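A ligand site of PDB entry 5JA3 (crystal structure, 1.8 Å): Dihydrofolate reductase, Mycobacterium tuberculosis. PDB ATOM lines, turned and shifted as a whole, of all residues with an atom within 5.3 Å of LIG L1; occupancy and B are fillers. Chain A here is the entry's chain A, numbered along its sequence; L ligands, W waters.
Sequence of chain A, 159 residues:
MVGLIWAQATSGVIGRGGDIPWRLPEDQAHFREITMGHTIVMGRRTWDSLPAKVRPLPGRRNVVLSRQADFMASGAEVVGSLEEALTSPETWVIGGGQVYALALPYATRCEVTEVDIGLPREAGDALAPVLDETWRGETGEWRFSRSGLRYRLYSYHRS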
ATOM      1  N   ILE A   5     -10.290   5.586  22.962  1.00  0.00           N
ATOM      2  CA  ILE A   5      -9.423   5.322  21.818  1.00  0.00           C
ATOM      3  C   ILE A   5     -10.279   4.831  20.666  1.00  0.00           C
ATOM      4  O   ILE A   5     -11.098   3.928  20.835  1.00  0.00           O
ATOM      5  CB  ILE A   5      -8.304   4.305  22.157  1.00  0.00           C
ATOM      6  CG1 ILE A   5      -7.424   4.016  20.933  1.00  0.00           C
ATOM      7  CG2 ILE A   5      -8.873   3.046  22.810  1.00  0.00           C
ATOM      8  CD1 ILE A   5      -6.155   3.235  21.314  1.00  0.00           C
ATOM      9  N   TRP A   6     -10.136   5.461  19.503  1.00  0.00           N
ATOM     10  CA  TRP A   6     -10.910   5.073  18.338  1.00  0.00           C
ATOM     11  C   TRP A   6     -10.139   5.392  17.056  1.00  0.00           C
ATOM     12  O   TRP A   6      -9.192   6.155  17.075  1.00  0.00           O
ATOM     13  CB  TRP A   6     -12.279   5.766  18.311  1.00  0.00           C
ATOM     14  CG  TRP A   6     -12.264   7.248  17.931  1.00  0.00           C
ATOM     15  CD1 TRP A   6     -12.181   7.773  16.661  1.00  0.00           C
ATOM     16  CD2 TRP A   6     -12.366   8.353  18.823  1.00  0.00           C
ATOM     17  NE1 TRP A   6     -12.216   9.149  16.728  1.00  0.00           N
ATOM     18  CE2 TRP A   6     -12.318   9.525  18.038  1.00  0.00           C
ATOM     19  CE3 TRP A   6     -12.477   8.472  20.212  1.00  0.00           C
ATOM     20  CZ2 TRP A   6     -12.398  10.796  18.603  1.00  0.00           C
ATOM     21  CZ3 TRP A   6     -12.533   9.749  20.775  1.00  0.00           C
ATOM     22  CH2 TRP A   6     -12.491  10.890  19.962  1.00  0.00           C
ATOM     23  N   ALA A   7     -10.607   4.798  15.952  1.00  0.00           N
ATOM     24  CA  ALA A   7     -10.100   5.101  14.612  1.00  0.00           C
ATOM     25  C   ALA A   7     -11.287   5.554  13.751  1.00  0.00           C
ATOM     26  O   ALA A   7     -12.336   4.903  13.747  1.00  0.00           O
ATOM     27  CB  ALA A   7      -9.414   3.885  14.011  1.00  0.00           C
ATOM     28  N   ASP A  19     -19.241  -3.421  11.352  1.00  0.00           N
ATOM     29  CA  ASP A  19     -17.793  -3.573  11.223  1.00  0.00           C
ATOM     30  C   ASP A  19     -17.059  -2.254  10.904  1.00  0.00           C
ATOM     31  O   ASP A  19     -17.672  -1.254  10.521  1.00  0.00           O
ATOM     32  CB  ASP A  19     -17.479  -4.622  10.156  1.00  0.00           C
ATOM     33  CG  ASP A  19     -16.137  -5.298  10.402  1.00  0.00           C
ATOM     34  OD1 ASP A  19     -15.367  -5.478   9.425  1.00  0.00           O
ATOM     35  OD2 ASP A  19     -15.862  -5.638  11.572  1.00  0.00           O
ATOM     36  N   ILE A  20     -15.748  -2.283  11.087  1.00  0.00           N
ATOM     37  CA  ILE A  20     -14.885  -1.153  10.748  1.00  0.00           C
ATOM     38  C   ILE A  20     -14.596  -1.209   9.248  1.00  0.00           C
ATOM     39  O   ILE A  20     -14.019  -2.177   8.767  1.00  0.00           O
ATOM     40  CB  ILE A  20     -13.580  -1.182  11.560  1.00  0.00           C
ATOM     41  CG1 ILE A  20     -13.905  -1.121  13.050  1.00  0.00           C
ATOM     42  CG2 ILE A  20     -12.676  -0.037  11.155  1.00  0.00           C
ATOM     43  CD1 ILE A  20     -12.693  -1.246  13.971  1.00  0.00           C
ATOM     44  N   ASP A  27      -2.800   0.400  12.917  1.00  0.00           N
ATOM     45  CA  ASP A  27      -3.717   0.900  13.932  1.00  0.00           C
ATOM     46  C   ASP A  27      -4.024  -0.157  14.987  1.00  0.00           C
ATOM     47  O   ASP A  27      -4.154   0.155  16.183  1.00  0.00           O
ATOM     48  CB  ASP A  27      -5.025   1.385  13.280  1.00  0.00           C
ATOM     49  CG  ASP A  27      -6.080   1.800  14.318  1.00  0.00           C
ATOM     50  OD1 ASP A  27      -5.880   2.810  15.005  1.00  0.00           O
ATOM     51  OD2 ASP A  27      -7.127   1.122  14.394  1.00  0.00           O
ATOM     52  N   GLN A  28      -4.172  -1.396  14.547  1.00  0.00           N
ATOM     53  CA  GLN A  28      -4.378  -2.517  15.454  1.00  0.00           C
ATOM     54  C   GLN A  28      -3.190  -2.642  16.421  1.00  0.00           C
ATOM     55  O   GLN A  28      -3.367  -2.836  17.625  1.00  0.00           O
ATOM     56  CB  GLN A  28      -4.580  -3.816  14.668  1.00  0.00           C
ATOM     57  CG  GLN A  28      -4.699  -5.066  15.499  1.00  0.00           C
ATOM     58  CD  GLN A  28      -5.429  -6.155  14.755  1.00  0.00           C
ATOM     59  OE1 GLN A  28      -6.361  -5.872  13.998  1.00  0.00           O
ATOM     60  NE2 GLN A  28      -5.013  -7.394  14.940  1.00  0.00           N
ATOM     61  N   HIS A  30      -1.212  -0.168  17.244  1.00  0.00           N
ATOM     62  CA  HIS A  30      -1.273   1.047  18.064  1.00  0.00           C
ATOM     63  C   HIS A  30      -2.271   0.878  19.205  1.00  0.00           C
ATOM     64  O   HIS A  30      -1.976   1.163  20.362  1.00  0.00           O
ATOM     65  CB  HIS A  30      -1.664   2.238  17.194  1.00  0.00           C
ATOM     66  CG  HIS A  30      -1.832   3.528  17.953  1.00  0.00           C
ATOM     67  ND1 HIS A  30      -3.030   4.205  18.015  1.00  0.00           N
ATOM     68  CD2 HIS A  30      -0.949   4.263  18.672  1.00  0.00           C
ATOM     69  CE1 HIS A  30      -2.877   5.303  18.743  1.00  0.00           C
ATOM     70  NE2 HIS A  30      -1.622   5.353  19.155  1.00  0.00           N
ATOM     71  N   PHE A  31      -3.466   0.422  18.852  1.00  0.00           N
ATOM     72  CA  PHE A  31      -4.501   0.074  19.816  1.00  0.00           C
ATOM     73  C   PHE A  31      -4.007  -0.963  20.837  1.00  0.00           C
ATOM     74  O   PHE A  31      -4.203  -0.797  22.056  1.00  0.00           O
ATOM     75  CB  PHE A  31      -5.736  -0.443  19.044  1.00  0.00           C
ATOM     76  CG  PHE A  31      -6.792  -1.074  19.899  1.00  0.00           C
ATOM     77  CD1 PHE A  31      -7.831  -0.316  20.440  1.00  0.00           C
ATOM     78  CD2 PHE A  31      -6.796  -2.446  20.107  1.00  0.00           C
ATOM     79  CE1 PHE A  31      -8.807  -0.910  21.208  1.00  0.00           C
ATOM     80  CE2 PHE A  31      -7.789  -3.040  20.877  1.00  0.00           C
ATOM     81  CZ  PHE A  31      -8.798  -2.267  21.418  1.00  0.00           C
ATOM     82  N   ARG A  32      -3.347  -2.004  20.367  1.00  0.00           N
ATOM     83  CA  ARG A  32      -2.819  -3.037  21.262  1.00  0.00           C
ATOM     84  C   ARG A  32      -1.833  -2.465  22.283  1.00  0.00           C
ATOM     85  O   ARG A  32      -1.908  -2.771  23.472  1.00  0.00           O
ATOM     86  CB  ARG A  32      -2.149  -4.157  20.466  1.00  0.00           C
ATOM     87  CG  ARG A  32      -1.816  -5.371  21.300  1.00  0.00           C
ATOM     88  CD  ARG A  32      -0.758  -6.275  20.650  1.00  0.00           C
ATOM     89  NE  ARG A  32      -0.016  -7.020  21.666  1.00  0.00           N
ATOM     90  CZ  ARG A  32       1.015  -6.528  22.356  1.00  0.00           C
ATOM     91  NH1 ARG A  32       1.433  -5.282  22.123  1.00  0.00           N
ATOM     92  NH2 ARG A  32       1.630  -7.268  23.276  1.00  0.00           N
ATOM     93  N   MET A  36      -3.021  -2.708  26.154  1.00  0.00           N
ATOM     94  CA  MET A  36      -2.527  -3.949  26.776  1.00  0.00           C
ATOM     95  C   MET A  36      -2.317  -3.818  28.269  1.00  0.00           C
ATOM     96  O   MET A  36      -1.762  -2.830  28.757  1.00  0.00           O
ATOM     97  CB  MET A  36      -1.216  -4.408  26.135  1.00  0.00           C
ATOM     98  CG  MET A  36      -0.733  -5.744  26.663  1.00  0.00           C
ATOM     99  SD  MET A  36      -1.885  -7.106  26.332  1.00  0.00           S
ATOM    100  CE  MET A  36      -2.345  -6.780  24.657  1.00  0.00           C
ATOM    101  N   THR A  46     -20.062  -3.678  20.104  1.00  0.00           N
ATOM    102  CA  THR A  46     -18.636  -3.748  19.829  1.00  0.00           C
ATOM    103  C   THR A  46     -18.122  -5.140  20.202  1.00  0.00           C
ATOM    104  O   THR A  46     -17.356  -5.737  19.455  1.00  0.00           O
ATOM    105  CB  THR A  46     -17.857  -2.649  20.585  1.00  0.00           C
ATOM    106  OG1 THR A  46     -18.177  -1.370  20.035  1.00  0.00           O
ATOM    107  CG2 THR A  46     -16.362  -2.852  20.439  1.00  0.00           C
ATOM    108  N   SER A  49     -18.944  -7.509  17.513  1.00  0.00           N
ATOM    109  CA  SER A  49     -18.164  -7.263  16.308  1.00  0.00           C
ATOM    110  C   SER A  49     -16.714  -7.708  16.431  1.00  0.00           C
ATOM    111  O   SER A  49     -15.982  -7.667  15.445  1.00  0.00           O
ATOM    112  CB  SER A  49     -18.185  -5.780  15.954  1.00  0.00           C
ATOM    113  OG  SER A  49     -17.224  -5.065  16.712  1.00  0.00           O
ATOM    114  N   LEU A  50     -16.257  -8.075  17.629  1.00  0.00           N
ATOM    115  CA  LEU A  50     -14.886  -8.560  17.756  1.00  0.00           C
ATOM    116  C   LEU A  50     -14.733  -9.858  16.967  1.00  0.00           C
ATOM    117  O   LEU A  50     -15.611 -10.724  17.056  1.00  0.00           O
ATOM    118  CB  LEU A  50     -14.505  -8.784  19.222  1.00  0.00           C
ATOM    119  CG  LEU A  50     -14.351  -7.535  20.080  1.00  0.00           C
ATOM    120  CD1 LEU A  50     -14.169  -7.935  21.552  1.00  0.00           C
ATOM    121  CD2 LEU A  50     -13.186  -6.683  19.596  1.00  0.00           C
ATOM    122  N   PRO A  51     -13.647  -9.996  16.190  1.00  0.00           N
ATOM    123  CA  PRO A  51     -13.362 -11.308  15.610  1.00  0.00           C
ATOM    124  C   PRO A  51     -13.353 -12.353  16.719  1.00  0.00           C
ATOM    125  O   PRO A  51     -12.764 -12.109  17.780  1.00  0.00           O
ATOM    126  CB  PRO A  51     -11.966 -11.129  15.010  1.00  0.00           C
ATOM    127  CG  PRO A  51     -11.846  -9.675  14.745  1.00  0.00           C
ATOM    128  CD  PRO A  51     -12.606  -9.008  15.866  1.00  0.00           C
ATOM    129  N   VAL A  54     -10.265 -13.159  18.973  1.00  0.00           N
ATOM    130  CA  VAL A  54      -9.801 -12.215  19.985  1.00  0.00           C
ATOM    131  C   VAL A  54     -10.977 -11.716  20.820  1.00  0.00           C
ATOM    132  O   VAL A  54     -11.038 -10.540  21.200  1.00  0.00           O
ATOM    133  CB  VAL A  54      -9.060 -11.025  19.344  1.00  0.00           C
ATOM    134  CG1 VAL A  54      -7.715 -11.474  18.789  1.00  0.00           C
ATOM    135  CG2 VAL A  54      -9.907 -10.368  18.273  1.00  0.00           C
ATOM    136  N   LEU A  57     -10.631  -9.768  24.154  1.00  0.00           N
ATOM    137  CA  LEU A  57      -9.282  -9.357  23.774  1.00  0.00           C
ATOM    138  C   LEU A  57      -8.262  -9.805  24.849  1.00  0.00           C
ATOM    139  O   LEU A  57      -8.439  -9.560  26.040  1.00  0.00           O
ATOM    140  CB  LEU A  57      -9.222  -7.847  23.565  1.00  0.00           C
ATOM    141  CG  LEU A  57      -9.984  -7.333  22.350  1.00  0.00           C
ATOM    142  CD1 LEU A  57     -10.260  -5.826  22.478  1.00  0.00           C
ATOM    143  CD2 LEU A  57      -9.204  -7.634  21.074  1.00  0.00           C
ATOM    144  N   ARG A  60      -6.151  -8.146  28.539  1.00  0.00           N
ATOM    145  CA  ARG A  60      -6.927  -7.004  29.007  1.00  0.00           C
ATOM    146  C   ARG A  60      -8.164  -7.491  29.760  1.00  0.00           C
ATOM    147  O   ARG A  60      -8.724  -8.553  29.437  1.00  0.00           O
ATOM    148  CB  ARG A  60      -7.321  -6.108  27.826  1.00  0.00           C
ATOM    149  CG  ARG A  60      -6.137  -5.281  27.312  1.00  0.00           C
ATOM    150  CD  ARG A  60      -6.157  -5.052  25.785  1.00  0.00           C
ATOM    151  NE  ARG A  60      -5.973  -6.289  25.029  1.00  0.00           N
ATOM    152  CZ  ARG A  60      -5.774  -6.350  23.718  1.00  0.00           C
ATOM    153  NH1 ARG A  60      -5.735  -5.234  22.994  1.00  0.00           N
ATOM    154  NH2 ARG A  60      -5.602  -7.522  23.125  1.00  0.00           N
ATOM    155  N   VAL A  93     -11.867   3.147  27.035  1.00  0.00           N
ATOM    156  CA  VAL A  93     -13.130   2.892  26.364  1.00  0.00           C
ATOM    157  C   VAL A  93     -12.875   2.677  24.874  1.00  0.00           C
ATOM    158  O   VAL A  93     -12.305   3.540  24.207  1.00  0.00           O
ATOM    159  CB  VAL A  93     -14.098   4.060  26.609  1.00  0.00           C
ATOM    160  CG1 VAL A  93     -15.340   3.909  25.749  1.00  0.00           C
ATOM    161  CG2 VAL A  93     -14.457   4.124  28.103  1.00  0.00           C
ATOM    162  N   ILE A  94     -13.254   1.517  24.349  1.00  0.00           N
ATOM    163  CA  ILE A  94     -12.759   1.110  23.031  1.00  0.00           C
ATOM    164  C   ILE A  94     -13.887   1.054  22.037  1.00  0.00           C
ATOM    165  O   ILE A  94     -13.718   0.619  20.904  1.00  0.00           O
ATOM    166  CB  ILE A  94     -12.057  -0.271  23.053  1.00  0.00           C
ATOM    167  CG1 ILE A  94     -13.055  -1.381  23.417  1.00  0.00           C
ATOM    168  CG2 ILE A  94     -10.922  -0.288  24.051  1.00  0.00           C
ATOM    169  CD1 ILE A  94     -12.663  -2.740  22.890  1.00  0.00           C
ATOM    170  N   GLY A  95     -15.080   1.452  22.419  1.00  0.00           N
ATOM    171  CA  GLY A  95     -16.107   0.954  21.566  1.00  0.00           C
ATOM    172  C   GLY A  95     -17.417   1.605  21.312  1.00  0.00           C
ATOM    173  O   GLY A  95     -18.230   1.823  22.192  1.00  0.00           O
ATOM    174  N   TYR A 100     -18.989   5.658  23.290  1.00  0.00           N
ATOM    175  CA  TYR A 100     -18.118   6.835  23.202  1.00  0.00           C
ATOM    176  C   TYR A 100     -18.837   8.083  23.690  1.00  0.00           C
ATOM    177  O   TYR A 100     -18.319   8.850  24.517  1.00  0.00           O
ATOM    178  CB  TYR A 100     -17.620   7.067  21.772  1.00  0.00           C
ATOM    179  CG  TYR A 100     -16.521   6.124  21.314  1.00  0.00           C
ATOM    180  CD1 TYR A 100     -15.543   5.664  22.178  1.00  0.00           C
ATOM    181  CD2 TYR A 100     -16.495   5.668  19.999  1.00  0.00           C
ATOM    182  CE1 TYR A 100     -14.520   4.786  21.727  1.00  0.00           C
ATOM    183  CE2 TYR A 100     -15.512   4.798  19.546  1.00  0.00           C
ATOM    184  CZ  TYR A 100     -14.534   4.352  20.407  1.00  0.00           C
ATOM    185  OH  TYR A 100     -13.567   3.473  19.924  1.00  0.00           O
ATOM    186  N   GLU A 111      -7.194   9.024  22.332  1.00  0.00           N
ATOM    187  CA  GLU A 111      -6.164   8.632  21.368  1.00  0.00           C
ATOM    188  C   GLU A 111      -6.868   8.284  20.075  1.00  0.00           C
ATOM    189  O   GLU A 111      -7.652   7.333  20.019  1.00  0.00           O
ATOM    190  CB  GLU A 111      -5.349   7.462  21.897  1.00  0.00           C
ATOM    191  CG  GLU A 111      -4.447   7.815  23.085  1.00  0.00           C
ATOM    192  CD  GLU A 111      -3.390   8.854  22.765  1.00  0.00           C
ATOM    193  OE1 GLU A 111      -3.014   9.020  21.586  1.00  0.00           O
ATOM    194  OE2 GLU A 111      -2.896   9.520  23.694  1.00  0.00           O
ATOM    195  N   THR A 113      -6.982   7.755  15.823  1.00  0.00           N
ATOM    196  CA  THR A 113      -6.389   7.471  14.532  1.00  0.00           C
ATOM    197  C   THR A 113      -7.302   8.027  13.458  1.00  0.00           C
ATOM    198  O   THR A 113      -8.498   7.707  13.429  1.00  0.00           O
ATOM    199  CB  THR A 113      -6.189   5.965  14.302  1.00  0.00           C
ATOM    200  OG1 THR A 113      -5.384   5.400  15.354  1.00  0.00           O
ATOM    201  CG2 THR A 113      -5.524   5.687  12.918  1.00  0.00           C
HETATM  202  C1  LIG L   1     -10.315   1.169  18.684  1.00  0.00           C
HETATM  203  C2  LIG L   1     -10.329   0.045  17.864  1.00  0.00           C
HETATM  204  C3  LIG L   1      -9.414  -0.022  16.813  1.00  0.00           C
HETATM  205  N1  LIG L   1      -8.559   0.985  16.628  1.00  0.00           N
HETATM  206  N2  LIG L   1      -9.433   2.146  18.453  1.00  0.00           N
HETATM  207  C4  LIG L   1      -8.016  -1.681  15.718  1.00  0.00           C
HETATM  208  C5  LIG L   1      -9.424  -1.128  15.953  1.00  0.00           C
HETATM  209  C6  LIG L   1      -8.557   2.054  17.436  1.00  0.00           C
HETATM  210  N3  LIG L   1      -7.674   3.028  17.219  1.00  0.00           N
HETATM  211  N4  LIG L   1     -11.199   1.226  19.708  1.00  0.00           N
HETATM  212  C7  LIG L   1     -11.250  -1.061  18.031  1.00  0.00           C
HETATM  213  C8  LIG L   1     -11.987  -2.080  18.071  1.00  0.00           C
HETATM  214  C9  LIG L   1     -12.767  -3.336  17.985  1.00  0.00           C
HETATM  215  C10 LIG L   1     -11.997  -4.252  17.214  1.00  0.00           C
HETATM  216  C11 LIG L   1     -10.749  -4.679  17.659  1.00  0.00           C
HETATM  217  C12 LIG L   1     -12.457  -4.687  15.979  1.00  0.00           C
HETATM  218  O1  LIG L   1     -13.684  -4.220  15.593  1.00  0.00           O
HETATM  219  C13 LIG L   1     -14.231  -4.885  14.443  1.00  0.00           C
HETATM  220  C14 LIG L   1     -11.696  -5.570  15.216  1.00  0.00           C
HETATM  221  C15 LIG L   1     -10.453  -6.008  15.673  1.00  0.00           C
HETATM  222  C16 LIG L   1      -9.964  -5.542  16.891  1.00  0.00           C
HETATM  223  C17 LIG L   1      -8.749  -5.981  17.416  1.00  0.00           C
HETATM  224  C18 LIG L   1      -8.126  -7.158  17.005  1.00  0.00           C
HETATM  225  C19 LIG L   1      -6.941  -7.584  17.617  1.00  0.00           C
HETATM  226  C20 LIG L   1      -6.377  -6.836  18.654  1.00  0.00           C
HETATM  227  C21 LIG L   1      -5.207  -7.217  19.314  1.00  0.00           C
HETATM  228  O2  LIG L   1      -4.834  -6.563  20.310  1.00  0.00           O
HETATM  229  O3  LIG L   1      -4.571  -8.231  18.977  1.00  0.00           O
HETATM  230  C22 LIG L   1      -7.006  -5.680  19.068  1.00  0.00           C
HETATM  231  C23 LIG L   1      -8.186  -5.260  18.461  1.00  0.00           C
HETATM  232  P1  LG2 L   2     -21.920   0.072  20.913  1.00  0.00           P
HETATM  233  O1  LG2 L   2     -21.752   1.478  21.370  1.00  0.00           O
HETATM  234  O2  LG2 L   2     -20.695  -0.728  20.549  1.00  0.00           O
HETATM  235  O3  LG2 L   2     -22.740  -0.800  22.003  1.00  0.00           O
HETATM  236  C1  LG2 L   2     -24.077  -0.359  22.051  1.00  0.00           C
HETATM  237  C2  LG2 L   2     -24.710  -1.235  23.151  1.00  0.00           C
HETATM  238  O4  LG2 L   2     -24.050  -1.013  24.389  1.00  0.00           O
HETATM  239  C3  LG2 L   2     -26.213  -0.946  23.383  1.00  0.00           C
HETATM  240  O5  LG2 L   2     -26.969  -1.597  22.446  1.00  0.00           O
HETATM  241  C4  LG2 L   2     -26.357  -1.638  24.780  1.00  0.00           C
HETATM  242  O6  LG2 L   2     -26.225  -2.958  24.761  1.00  0.00           O
HETATM  243  C5  LG2 L   2     -25.015  -1.154  25.432  1.00  0.00           C
HETATM  244  N1  LG2 L   2     -25.140   0.108  26.130  1.00  0.00           N
HETATM  245  C6  LG2 L   2     -24.953   1.409  25.618  1.00  0.00           C
HETATM  246  N2  LG2 L   2     -25.148   2.376  26.552  1.00  0.00           N
HETATM  247  C7  LG2 L   2     -25.473   1.652  27.703  1.00  0.00           C
HETATM  248  C8  LG2 L   2     -25.783   2.062  29.004  1.00  0.00           C
HETATM  249  N3  LG2 L   2     -25.820   3.400  29.333  1.00  0.00           N
HETATM  250  N4  LG2 L   2     -26.070   1.146  29.989  1.00  0.00           N
HETATM  251  C9  LG2 L   2     -26.026  -0.174  29.599  1.00  0.00           C
HETATM  252  N5  LG2 L   2     -25.748  -0.706  28.403  1.00  0.00           N
HETATM  253  C10 LG2 L   2     -25.466   0.250  27.450  1.00  0.00           C
HETATM  254  O7  LG2 L   2     -22.902   0.059  19.522  1.00  0.00           O
HETATM  255  P2  LG2 L   2     -22.588   1.117  18.327  1.00  0.00           P
HETATM  256  O8  LG2 L   2     -23.390   0.602  17.200  1.00  0.00           O
HETATM  257  O9  LG2 L   2     -22.617   2.580  18.655  1.00  0.00           O
HETATM  258  O10 LG2 L   2     -20.979   0.933  17.774  1.00  0.00           O
HETATM  259  C11 LG2 L   2     -20.816  -0.277  17.129  1.00  0.00           C
HETATM  260  C12 LG2 L   2     -20.057   0.017  15.813  1.00  0.00           C
HETATM  261  O11 LG2 L   2     -18.815   0.722  16.111  1.00  0.00           O
HETATM  262  C13 LG2 L   2     -19.671  -1.299  15.041  1.00  0.00           C
HETATM  263  O12 LG2 L   2     -19.802  -1.078  13.668  1.00  0.00           O
HETATM  264  C14 LG2 L   2     -18.201  -1.460  15.368  1.00  0.00           C
HETATM  265  O13 LG2 L   2     -17.507  -2.139  14.346  1.00  0.00           O
HETATM  266  C15 LG2 L   2     -17.760   0.043  15.398  1.00  0.00           C
HETATM  267  N6  LG2 L   2     -16.503   0.237  16.157  1.00  0.00           N
HETATM  268  C16 LG2 L   2     -15.476   1.015  15.632  1.00  0.00           C
HETATM  269  C17 LG2 L   2     -14.373   1.307  16.356  1.00  0.00           C
HETATM  270  C18 LG2 L   2     -13.333   2.155  15.743  1.00  0.00           C
HETATM  271  O14 LG2 L   2     -12.415   2.686  16.381  1.00  0.00           O
HETATM  272  N7  LG2 L   2     -13.381   2.396  14.375  1.00  0.00           N
HETATM  273  C19 LG2 L   2     -14.185   0.818  17.777  1.00  0.00           C
HETATM  274  C20 LG2 L   2     -15.295  -0.074  18.210  1.00  0.00           C
HETATM  275  C21 LG2 L   2     -16.369  -0.319  17.450  1.00  0.00           C
HETATM  276  P3  LG2 L   2     -27.746  -3.943  24.649  1.00  0.00           P
HETATM  277  O15 LG2 L   2     -28.109  -3.570  23.239  1.00  0.00           O
HETATM  278  O16 LG2 L   2     -27.214  -5.356  24.884  1.00  0.00           O
HETATM  279  O17 LG2 L   2     -28.527  -3.309  25.756  1.00  0.00           O
HETATM  280  O   HOH W   1      -6.082   5.477  18.036  1.00  0.00           O
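Residues that only touch LIG L1: Phe 31 (3.3 Å), Gln 28 (3.3 Å), Asp 19 (3.4 Å), Arg 32 (3.4 Å), Ser 49 (3.4 Å), Ile 20 (3.5 Å), Leu 57 (3.6 Å), Leu 50 (3.6 Å), Pro 51 (3.6 Å), Ala 7 (3.7 Å), Thr 113 (3.8 Å) and Val 54 (3.9 Å).
Within 4 Å of LIG L1: Ile 5, Trp 6, Ala 7, Asp 19, Ile 20, Asp 27, Gln 28, Phe 31, Arg 32, Ser 49, Leu 50, Pro 51, Val 54, Leu 57, Arg 60, Ile 94, Tyr 100 and Thr 113.
OD2 of Asp 27 is in hydrogen-bond range of N1 of LIG L1, 2.7 Å away.
A nitrogen (N4) of LIG L1 is in hydrogen-bond range of the backbone carbonyl oxygen (O) of Ile 94, 2.9 Å away.
N4 of LIG L1 sits at hydrogen-bond distance from O of Ile 5 (2.9 Å).
NH2 of Arg 60 lies within salt-bridge range of O2 of LIG L1, at 3.1 Å.
OH of Tyr 100 sits at hydrogen-bond distance from N4 of LIG L1 (3.3 Å).
A nitrogen (N3) of LIG L1 sits close to the backbone carbonyl oxygen of Trp 6.
N of Asp 19 is in hydrogen-bond range of O12 of LG2 L2 (3.3 Å).
O14 of LG2 L2 is in hydrogen-bond range of N of Ala 7 (2.8 Å).
A nitrogen (N7) of LG2 L2 is in hydrogen-bond range of the backbone carbonyl oxygen (O) of Ala 7.
The backbone NH (N) of Thr 46 lies within hydrogen-bond range of an oxygen (O2) of LG2 L2 (3.0 Å).
OG1 of Thr 46 is in hydrogen-bond range of O2 of LG2 L2.
Water W1 lies within hydrogen-bond range of OG1 of Thr 113, N3 of LIG L1, O of Glu 111, ND1 of His 30 and O of Trp 6.
OD1 of Asp 27 sits at hydrogen-bond distance from OG1 of Thr 113 (2.7 Å).
O of Ile 94 is in hydrogen-bond range of OH of Tyr 100.
O of Ile 5 is in hydrogen-bond range of OH of Tyr 100 (2.7 Å).
The backbone carbonyl oxygen (O) of Val 93 sits at hydrogen-bond distance from the backbone NH (N) of Ile 5, at 3.1 Å.
The backbone carbonyl oxygen (O) of Trp 6 sits at hydrogen-bond distance from the backbone NH (N) of Thr 113, at 3.0 Å.
The backbone NH of Trp 6 lies within hydrogen-bond range of the backbone carbonyl oxygen of Glu 111 (3.2 Å).
O of Thr 46 lies within hydrogen-bond range of OG of Ser 49 (2.8 Å).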
